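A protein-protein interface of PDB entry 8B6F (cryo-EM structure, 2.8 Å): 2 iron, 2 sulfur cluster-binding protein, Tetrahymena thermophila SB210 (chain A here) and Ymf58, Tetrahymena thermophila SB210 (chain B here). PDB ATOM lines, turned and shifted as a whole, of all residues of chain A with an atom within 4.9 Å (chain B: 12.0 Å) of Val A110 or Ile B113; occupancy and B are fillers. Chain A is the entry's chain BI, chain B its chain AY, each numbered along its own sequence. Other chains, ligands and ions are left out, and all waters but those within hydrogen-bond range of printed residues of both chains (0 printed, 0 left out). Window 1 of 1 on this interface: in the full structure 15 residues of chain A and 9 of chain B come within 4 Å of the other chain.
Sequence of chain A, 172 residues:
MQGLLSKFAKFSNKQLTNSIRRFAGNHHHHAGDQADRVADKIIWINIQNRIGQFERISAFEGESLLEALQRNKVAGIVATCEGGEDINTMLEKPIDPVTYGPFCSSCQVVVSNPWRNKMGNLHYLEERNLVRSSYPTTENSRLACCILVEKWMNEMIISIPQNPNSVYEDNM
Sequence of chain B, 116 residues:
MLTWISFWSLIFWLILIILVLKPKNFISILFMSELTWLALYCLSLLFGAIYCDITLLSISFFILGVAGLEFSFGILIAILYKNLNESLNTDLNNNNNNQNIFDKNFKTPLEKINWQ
Among the printed residues, pairs that only touch across the chains: Thr A138 with Thr B108, Asn A113 with Asn B114, Asn A140 with Ile B113, Ser A112 with Gln B116, Pro A161 with Thr B108, Thr A138 with Ile B113, Ile A157 with Trp B115, Ser A159 with Leu B110, Val A110 with Leu B110, Val A110 with Ile B113, Pro A161 with Leu B110, Ser A159 with Trp B115, Pro A161 with Pro B109, Ser A112 with Ile B113 and Glu A139 with Ile B113.
Val A110 touches just these residues of chain B: Leu B110 (3.7 Å) and Ile B113 (3.7 Å). Of the printed residues of chain A, Ile B113 touches Val A110, Ser A112, Thr A138, Glu A139 and Asn A140. No residue of chain B comes within 4 Å of Val A111. Of chain B, only Thr B108 and Ile B113 come within 4 Å of Thr A138. Ser A141 touches none of the printed residues of chain B. Of chain B, only Leu B110 and Trp B115 come within 4 Å of Ser A159. Of chain B, only Thr B108, Pro B109 and Leu B110 come within 4 Å of Pro A161. Of the printed residues of chain A, Trp B115 touches Ser A112 (3.2 Å), Ile A157 (3.7 Å) and Ser A159 (3.8 Å). Of the printed residues of chain B, Asn A113 touches Asn B114 (3.3 Å). Of the printed residues of chain A, Asn B114 touches Asn A113 and Asn A140. Lys B107 touches none of the printed residues of chain A.
N of Ser A159 sits at hydrogen-bond distance from O of Val A110. O of Val A111 lies within hydrogen-bond range of ND2 of Asn A140 (2.7 Å). The backbone NH (N) of Ser A112 is in hydrogen-bond range of the backbone carbonyl oxygen (O) of Ile A157, 3.1 Å away. The side-chain hydroxyl (OG1) of Thr A138 sits at hydrogen-bond distance from the side-chain hydroxyl (OG) of Ser A141, 2.6 Å away.
The side-chain amide oxygen (OD1) of Asn B114 lies within hydrogen-bond range of the side-chain amide nitrogen (ND2) of Asn A140 (3.3 Å). The side-chain hydroxyl (OG) of Ser A112 sits at hydrogen-bond distance from the backbone NH (N) of Trp B115, at 3.2 Å.
Of the 14 printed residues of chain A, 9 touch a printed residue of chain B. Along chain A the printed residues that touch a printed residue of chain B span positions 110 to 161. Hydrophobic or aromatic side chains of chain B within 4 Å of the printed part of chain A: Pro B109, Leu B110, Ile B113 and Trp B115. Among the printed residues, 17 pairs touch across the chains. Among the printed residues, no Asp or Glu carboxylate lies within 4 Å of a Lys or Arg side-chain nitrogen of the other chain.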
ATOM      1  N   GLN A 108     -22.048 -12.106  19.536  1.00  0.00           N
ATOM      2  CA  GLN A 108     -21.063 -11.550  18.621  1.00  0.00           C
ATOM      3  C   GLN A 108     -20.123 -12.630  18.102  1.00  0.00           C
ATOM      4  O   GLN A 108     -19.688 -13.511  18.846  1.00  0.00           O
ATOM      5  CB  GLN A 108     -20.252 -10.457  19.311  1.00  0.00           C
ATOM      6  CG  GLN A 108     -21.089  -9.341  19.894  1.00  0.00           C
ATOM      7  CD  GLN A 108     -20.254  -8.333  20.650  1.00  0.00           C
ATOM      8  OE1 GLN A 108     -20.526  -8.036  21.810  1.00  0.00           O
ATOM      9  NE2 GLN A 108     -19.230  -7.798  19.993  1.00  0.00           N
ATOM     10  N   VAL A 109     -19.809 -12.554  16.812  1.00  0.00           N
ATOM     11  CA  VAL A 109     -18.847 -13.443  16.173  1.00  0.00           C
ATOM     12  C   VAL A 109     -17.978 -12.613  15.240  1.00  0.00           C
ATOM     13  O   VAL A 109     -18.471 -11.711  14.555  1.00  0.00           O
ATOM     14  CB  VAL A 109     -19.542 -14.588  15.405  1.00  0.00           C
ATOM     15  CG1 VAL A 109     -20.385 -15.427  16.350  1.00  0.00           C
ATOM     16  CG2 VAL A 109     -20.397 -14.037  14.276  1.00  0.00           C
ATOM     17  N   VAL A 110     -16.683 -12.908  15.220  1.00  0.00           N
ATOM     18  CA  VAL A 110     -15.743 -12.226  14.338  1.00  0.00           C
ATOM     19  C   VAL A 110     -15.634 -13.036  13.053  1.00  0.00           C
ATOM     20  O   VAL A 110     -15.264 -14.214  13.085  1.00  0.00           O
ATOM     21  CB  VAL A 110     -14.371 -12.061  15.007  1.00  0.00           C
ATOM     22  CG1 VAL A 110     -13.433 -11.274  14.110  1.00  0.00           C
ATOM     23  CG2 VAL A 110     -14.514 -11.381  16.356  1.00  0.00           C
ATOM     24  N   VAL A 111     -15.951 -12.407  11.924  1.00  0.00           N
ATOM     25  CA  VAL A 111     -15.975 -13.073  10.627  1.00  0.00           C
ATOM     26  C   VAL A 111     -14.748 -12.654   9.833  1.00  0.00           C
ATOM     27  O   VAL A 111     -14.339 -11.487   9.868  1.00  0.00           O
ATOM     28  CB  VAL A 111     -17.269 -12.745   9.858  1.00  0.00           C
ATOM     29  CG1 VAL A 111     -17.338 -13.531   8.558  1.00  0.00           C
ATOM     30  CG2 VAL A 111     -18.488 -13.034  10.715  1.00  0.00           C
ATOM     31  N   SER A 112     -14.160 -13.604   9.113  1.00  0.00           N
ATOM     32  CA  SER A 112     -12.980 -13.314   8.314  1.00  0.00           C
ATOM     33  C   SER A 112     -13.327 -12.367   7.169  1.00  0.00           C
ATOM     34  O   SER A 112     -14.450 -12.354   6.660  1.00  0.00           O
ATOM     35  CB  SER A 112     -12.379 -14.606   7.765  1.00  0.00           C
ATOM     36  OG  SER A 112     -11.139 -14.356   7.129  1.00  0.00           O
ATOM     37  N   ASN A 113     -12.337 -11.573   6.764  1.00  0.00           N
ATOM     38  CA  ASN A 113     -12.597 -10.482   5.828  1.00  0.00           C
ATOM     39  C   ASN A 113     -13.228 -10.928   4.516  1.00  0.00           C
ATOM     40  O   ASN A 113     -14.136 -10.227   4.037  1.00  0.00           O
ATOM     41  CB  ASN A 113     -11.298  -9.719   5.554  1.00  0.00           C
ATOM     42  CG  ASN A 113     -11.526  -8.476   4.729  1.00  0.00           C
ATOM     43  OD1 ASN A 113     -11.495  -8.518   3.500  1.00  0.00           O
ATOM     44  ND2 ASN A 113     -11.769  -7.358   5.401  1.00  0.00           N
ATOM     45  N   THR A 138     -14.572  -5.923  17.504  1.00  0.00           N
ATOM     46  CA  THR A 138     -13.729  -5.792  16.328  1.00  0.00           C
ATOM     47  C   THR A 138     -14.549  -5.260  15.161  1.00  0.00           C
ATOM     48  O   THR A 138     -15.775  -5.387  15.124  1.00  0.00           O
ATOM     49  CB  THR A 138     -13.098  -7.129  15.933  1.00  0.00           C
ATOM     50  OG1 THR A 138     -14.127  -8.084  15.649  1.00  0.00           O
ATOM     51  CG2 THR A 138     -12.231  -7.649  17.047  1.00  0.00           C
ATOM     52  N   GLU A 139     -13.849  -4.652  14.203  1.00  0.00           N
ATOM     53  CA  GLU A 139     -14.513  -4.143  13.009  1.00  0.00           C
ATOM     54  C   GLU A 139     -15.194  -5.252  12.219  1.00  0.00           C
ATOM     55  O   GLU A 139     -16.117  -4.970  11.447  1.00  0.00           O
ATOM     56  CB  GLU A 139     -13.513  -3.398  12.119  1.00  0.00           C
ATOM     57  CG  GLU A 139     -12.435  -4.267  11.477  1.00  0.00           C
ATOM     58  CD  GLU A 139     -11.364  -4.707  12.456  1.00  0.00           C
ATOM     59  OE1 GLU A 139     -11.456  -4.343  13.646  1.00  0.00           O
ATOM     60  OE2 GLU A 139     -10.427  -5.415  12.034  1.00  0.00           O
ATOM     61  N   ASN A 140     -14.762  -6.501  12.388  1.00  0.00           N
ATOM     62  CA  ASN A 140     -15.377  -7.640  11.720  1.00  0.00           C
ATOM     63  C   ASN A 140     -16.469  -8.302  12.550  1.00  0.00           C
ATOM     64  O   ASN A 140     -17.047  -9.296  12.102  1.00  0.00           O
ATOM     65  CB  ASN A 140     -14.312  -8.683  11.373  1.00  0.00           C
ATOM     66  CG  ASN A 140     -13.443  -8.265  10.207  1.00  0.00           C
ATOM     67  OD1 ASN A 140     -13.337  -7.084   9.890  1.00  0.00           O
ATOM     68  ND2 ASN A 140     -12.822  -9.239   9.556  1.00  0.00           N
ATOM     69  N   SER A 141     -16.767  -7.784  13.738  1.00  0.00           N
ATOM     70  CA  SER A 141     -17.767  -8.403  14.595  1.00  0.00           C
ATOM     71  C   SER A 141     -19.158  -8.287  13.986  1.00  0.00           C
ATOM     72  O   SER A 141     -19.488  -7.312  13.307  1.00  0.00           O
ATOM     73  CB  SER A 141     -17.766  -7.768  15.984  1.00  0.00           C
ATOM     74  OG  SER A 141     -16.519  -7.940  16.624  1.00  0.00           O
ATOM     75  N   ILE A 157     -14.835 -18.837   7.766  1.00  0.00           N
ATOM     76  CA  ILE A 157     -14.052 -18.917   8.993  1.00  0.00           C
ATOM     77  C   ILE A 157     -14.479 -17.784   9.914  1.00  0.00           C
ATOM     78  O   ILE A 157     -14.522 -16.621   9.498  1.00  0.00           O
ATOM     79  CB  ILE A 157     -12.546 -18.841   8.695  1.00  0.00           C
ATOM     80  CG1 ILE A 157     -12.115 -20.027   7.827  1.00  0.00           C
ATOM     81  CG2 ILE A 157     -11.749 -18.797   9.991  1.00  0.00           C
ATOM     82  CD1 ILE A 157     -10.690 -19.935   7.319  1.00  0.00           C
ATOM     83  N   ILE A 158     -14.796 -18.121  11.164  1.00  0.00           N
ATOM     84  CA  ILE A 158     -15.164 -17.139  12.177  1.00  0.00           C
ATOM     85  C   ILE A 158     -14.437 -17.487  13.470  1.00  0.00           C
ATOM     86  O   ILE A 158     -13.904 -18.584  13.636  1.00  0.00           O
ATOM     87  CB  ILE A 158     -16.688 -17.076  12.416  1.00  0.00           C
ATOM     88  CG1 ILE A 158     -17.188 -18.384  13.038  1.00  0.00           C
ATOM     89  CG2 ILE A 158     -17.409 -16.787  11.107  1.00  0.00           C
ATOM     90  CD1 ILE A 158     -18.696 -18.463  13.221  1.00  0.00           C
ATOM     91  N   SER A 159     -14.417 -16.527  14.390  1.00  0.00           N
ATOM     92  CA  SER A 159     -13.886 -16.724  15.730  1.00  0.00           C
ATOM     93  C   SER A 159     -14.960 -16.337  16.732  1.00  0.00           C
ATOM     94  O   SER A 159     -15.713 -15.388  16.501  1.00  0.00           O
ATOM     95  CB  SER A 159     -12.620 -15.892  15.970  1.00  0.00           C
ATOM     96  OG  SER A 159     -11.608 -16.212  15.032  1.00  0.00           O
ATOM     97  N   PRO A 161     -14.961 -15.476  20.553  1.00  0.00           N
ATOM     98  CA  PRO A 161     -14.584 -15.210  21.945  1.00  0.00           C
ATOM     99  C   PRO A 161     -15.799 -15.294  22.856  1.00  0.00           C
ATOM    100  O   PRO A 161     -16.939 -15.441  22.414  1.00  0.00           O
ATOM    101  CB  PRO A 161     -14.001 -13.794  21.897  1.00  0.00           C
ATOM    102  CG  PRO A 161     -13.602 -13.592  20.476  1.00  0.00           C
ATOM    103  CD  PRO A 161     -14.592 -14.365  19.662  1.00  0.00           C
ATOM    104  N   PHE B 106      -7.829  -2.261  25.903  1.00  0.00           N
ATOM    105  CA  PHE B 106      -8.353  -3.620  25.884  1.00  0.00           C
ATOM    106  C   PHE B 106      -8.569  -4.069  24.448  1.00  0.00           C
ATOM    107  O   PHE B 106      -9.016  -3.289  23.603  1.00  0.00           O
ATOM    108  CB  PHE B 106      -9.672  -3.725  26.661  1.00  0.00           C
ATOM    109  CG  PHE B 106      -9.527  -3.529  28.143  1.00  0.00           C
ATOM    110  CD1 PHE B 106      -8.434  -4.036  28.826  1.00  0.00           C
ATOM    111  CD2 PHE B 106     -10.493  -2.840  28.855  1.00  0.00           C
ATOM    112  CE1 PHE B 106      -8.307  -3.856  30.189  1.00  0.00           C
ATOM    113  CE2 PHE B 106     -10.370  -2.658  30.217  1.00  0.00           C
ATOM    114  CZ  PHE B 106      -9.276  -3.165  30.884  1.00  0.00           C
ATOM    115  N   LYS B 107      -8.252  -5.333  24.184  1.00  0.00           N
ATOM    116  CA  LYS B 107      -8.457  -5.951  22.885  1.00  0.00           C
ATOM    117  C   LYS B 107      -9.284  -7.213  23.065  1.00  0.00           C
ATOM    118  O   LYS B 107      -9.321  -7.808  24.144  1.00  0.00           O
ATOM    119  CB  LYS B 107      -7.128  -6.308  22.202  1.00  0.00           C
ATOM    120  CG  LYS B 107      -6.252  -5.122  21.854  1.00  0.00           C
ATOM    121  CD  LYS B 107      -4.897  -5.578  21.336  1.00  0.00           C
ATOM    122  CE  LYS B 107      -4.063  -4.409  20.836  1.00  0.00           C
ATOM    123  NZ  LYS B 107      -3.966  -3.308  21.834  1.00  0.00           N
ATOM    124  N   THR B 108      -9.953  -7.618  21.994  1.00  0.00           N
ATOM    125  CA  THR B 108     -10.646  -8.895  22.015  1.00  0.00           C
ATOM    126  C   THR B 108      -9.623 -10.017  22.170  1.00  0.00           C
ATOM    127  O   THR B 108      -8.522  -9.933  21.614  1.00  0.00           O
ATOM    128  CB  THR B 108     -11.452  -9.096  20.733  1.00  0.00           C
ATOM    129  OG1 THR B 108     -12.114 -10.366  20.774  1.00  0.00           O
ATOM    130  CG2 THR B 108     -10.542  -9.052  19.517  1.00  0.00           C
ATOM    131  N   PRO B 109      -9.939 -11.077  22.909  1.00  0.00           N
ATOM    132  CA  PRO B 109      -8.956 -12.151  23.087  1.00  0.00           C
ATOM    133  C   PRO B 109      -8.780 -12.984  21.828  1.00  0.00           C
ATOM    134  O   PRO B 109      -9.170 -14.155  21.784  1.00  0.00           O
ATOM    135  CB  PRO B 109      -9.541 -12.971  24.243  1.00  0.00           C
ATOM    136  CG  PRO B 109     -10.996 -12.755  24.145  1.00  0.00           C
ATOM    137  CD  PRO B 109     -11.189 -11.352  23.639  1.00  0.00           C
ATOM    138  N   LEU B 110      -8.195 -12.383  20.796  1.00  0.00           N
ATOM    139  CA  LEU B 110      -7.924 -13.051  19.533  1.00  0.00           C
ATOM    140  C   LEU B 110      -6.498 -12.751  19.100  1.00  0.00           C
ATOM    141  O   LEU B 110      -5.836 -11.860  19.637  1.00  0.00           O
ATOM    142  CB  LEU B 110      -8.906 -12.614  18.438  1.00  0.00           C
ATOM    143  CG  LEU B 110     -10.356 -13.075  18.589  1.00  0.00           C
ATOM    144  CD1 LEU B 110     -11.199 -12.516  17.461  1.00  0.00           C
ATOM    145  CD2 LEU B 110     -10.449 -14.592  18.618  1.00  0.00           C
ATOM    146  N   GLU B 111      -6.029 -13.512  18.116  1.00  0.00           N
ATOM    147  CA  GLU B 111      -4.694 -13.346  17.558  1.00  0.00           C
ATOM    148  C   GLU B 111      -4.702 -12.794  16.143  1.00  0.00           C
ATOM    149  O   GLU B 111      -3.813 -12.021  15.786  1.00  0.00           O
ATOM    150  CB  GLU B 111      -3.950 -14.688  17.576  1.00  0.00           C
ATOM    151  CG  GLU B 111      -2.527 -14.618  17.043  1.00  0.00           C
ATOM    152  CD  GLU B 111      -2.430 -14.963  15.570  1.00  0.00           C
ATOM    153  OE1 GLU B 111      -3.068 -15.950  15.146  1.00  0.00           O
ATOM    154  OE2 GLU B 111      -1.718 -14.248  14.836  1.00  0.00           O
ATOM    155  N   LYS B 112      -5.687 -13.165  15.331  1.00  0.00           N
ATOM    156  CA  LYS B 112      -5.784 -12.676  13.963  1.00  0.00           C
ATOM    157  C   LYS B 112      -7.253 -12.527  13.603  1.00  0.00           C
ATOM    158  O   LYS B 112      -8.031 -13.468  13.775  1.00  0.00           O
ATOM    159  CB  LYS B 112      -5.085 -13.626  12.985  1.00  0.00           C
ATOM    160  CG  LYS B 112      -5.621 -15.047  13.023  1.00  0.00           C
ATOM    161  CD  LYS B 112      -4.738 -16.001  12.239  1.00  0.00           C
ATOM    162  CE  LYS B 112      -4.709 -15.645  10.766  1.00  0.00           C
ATOM    163  NZ  LYS B 112      -3.985 -16.669   9.960  1.00  0.00           N
ATOM    164  N   ILE B 113      -7.625 -11.344  13.116  1.00  0.00           N
ATOM    165  CA  ILE B 113      -9.009 -11.114  12.717  1.00  0.00           C
ATOM    166  C   ILE B 113      -9.275 -11.684  11.330  1.00  0.00           C
ATOM    167  O   ILE B 113     -10.383 -12.158  11.054  1.00  0.00           O
ATOM    168  CB  ILE B 113      -9.339  -9.612  12.773  1.00  0.00           C
ATOM    169  CG1 ILE B 113      -9.060  -9.042  14.170  1.00  0.00           C
ATOM    170  CG2 ILE B 113     -10.788  -9.365  12.379  1.00  0.00           C
ATOM    171  CD1 ILE B 113      -9.850  -9.694  15.286  1.00  0.00           C
ATOM    172  N   ASN B 114      -8.284 -11.652  10.444  1.00  0.00           N
ATOM    173  CA  ASN B 114      -8.428 -12.114   9.071  1.00  0.00           C
ATOM    174  C   ASN B 114      -7.574 -13.354   8.861  1.00  0.00           C
ATOM    175  O   ASN B 114      -6.377 -13.347   9.161  1.00  0.00           O
ATOM    176  CB  ASN B 114      -8.016 -11.022   8.081  1.00  0.00           C
ATOM    177  CG  ASN B 114      -8.819  -9.751   8.249  1.00  0.00           C
ATOM    178  OD1 ASN B 114      -9.598  -9.618   9.190  1.00  0.00           O
ATOM    179  ND2 ASN B 114      -8.626  -8.804   7.342  1.00  0.00           N
ATOM    180  N   TRP B 115      -8.194 -14.415   8.347  1.00  0.00           N
ATOM    181  CA  TRP B 115      -7.497 -15.661   8.064  1.00  0.00           C
ATOM    182  C   TRP B 115      -7.169 -15.842   6.592  1.00  0.00           C
ATOM    183  O   TRP B 115      -6.119 -16.404   6.268  1.00  0.00           O
ATOM    184  CB  TRP B 115      -8.335 -16.853   8.539  1.00  0.00           C
ATOM    185  CG  TRP B 115      -8.497 -16.911  10.023  1.00  0.00           C
ATOM    186  CD1 TRP B 115      -9.338 -16.158  10.785  1.00  0.00           C
ATOM    187  CD2 TRP B 115      -7.796 -17.771  10.928  1.00  0.00           C
ATOM    188  NE1 TRP B 115      -9.206 -16.495  12.108  1.00  0.00           N
ATOM    189  CE2 TRP B 115      -8.265 -17.483  12.224  1.00  0.00           C
ATOM    190  CE3 TRP B 115      -6.818 -18.757  10.767  1.00  0.00           C
ATOM    191  CZ2 TRP B 115      -7.790 -18.145  13.352  1.00  0.00           C
ATOM    192  CZ3 TRP B 115      -6.347 -19.414  11.888  1.00  0.00           C
ATOM    193  CH2 TRP B 115      -6.832 -19.105  13.166  1.00  0.00           C
ATOM    194  N   GLN B 116      -8.037 -15.377   5.701  1.00  0.00           N
ATOM    195  CA  GLN B 116      -7.823 -15.512   4.268  1.00  0.00           C
ATOM    196  C   GLN B 116      -7.813 -14.137   3.610  1.00  0.00           C
ATOM    197  O   GLN B 116      -7.254 -13.953   2.529  1.00  0.00           O
ATOM    198  CB  GLN B 116      -8.906 -16.399   3.650  1.00  0.00           C
ATOM    199  CG  GLN B 116      -8.907 -16.426   2.130  1.00  0.00           C
ATOM    200  CD  GLN B 116      -9.928 -17.393   1.572  1.00  0.00           C
ATOM    201  OE1 GLN B 116     -10.394 -18.292   2.268  1.00  0.00           O
ATOM    202  NE2 GLN B 116     -10.287 -17.209   0.306  1.00  0.00           N
ATOM    203  OXT GLN B 116      -8.362 -13.175   4.148  1.00  0.00           O
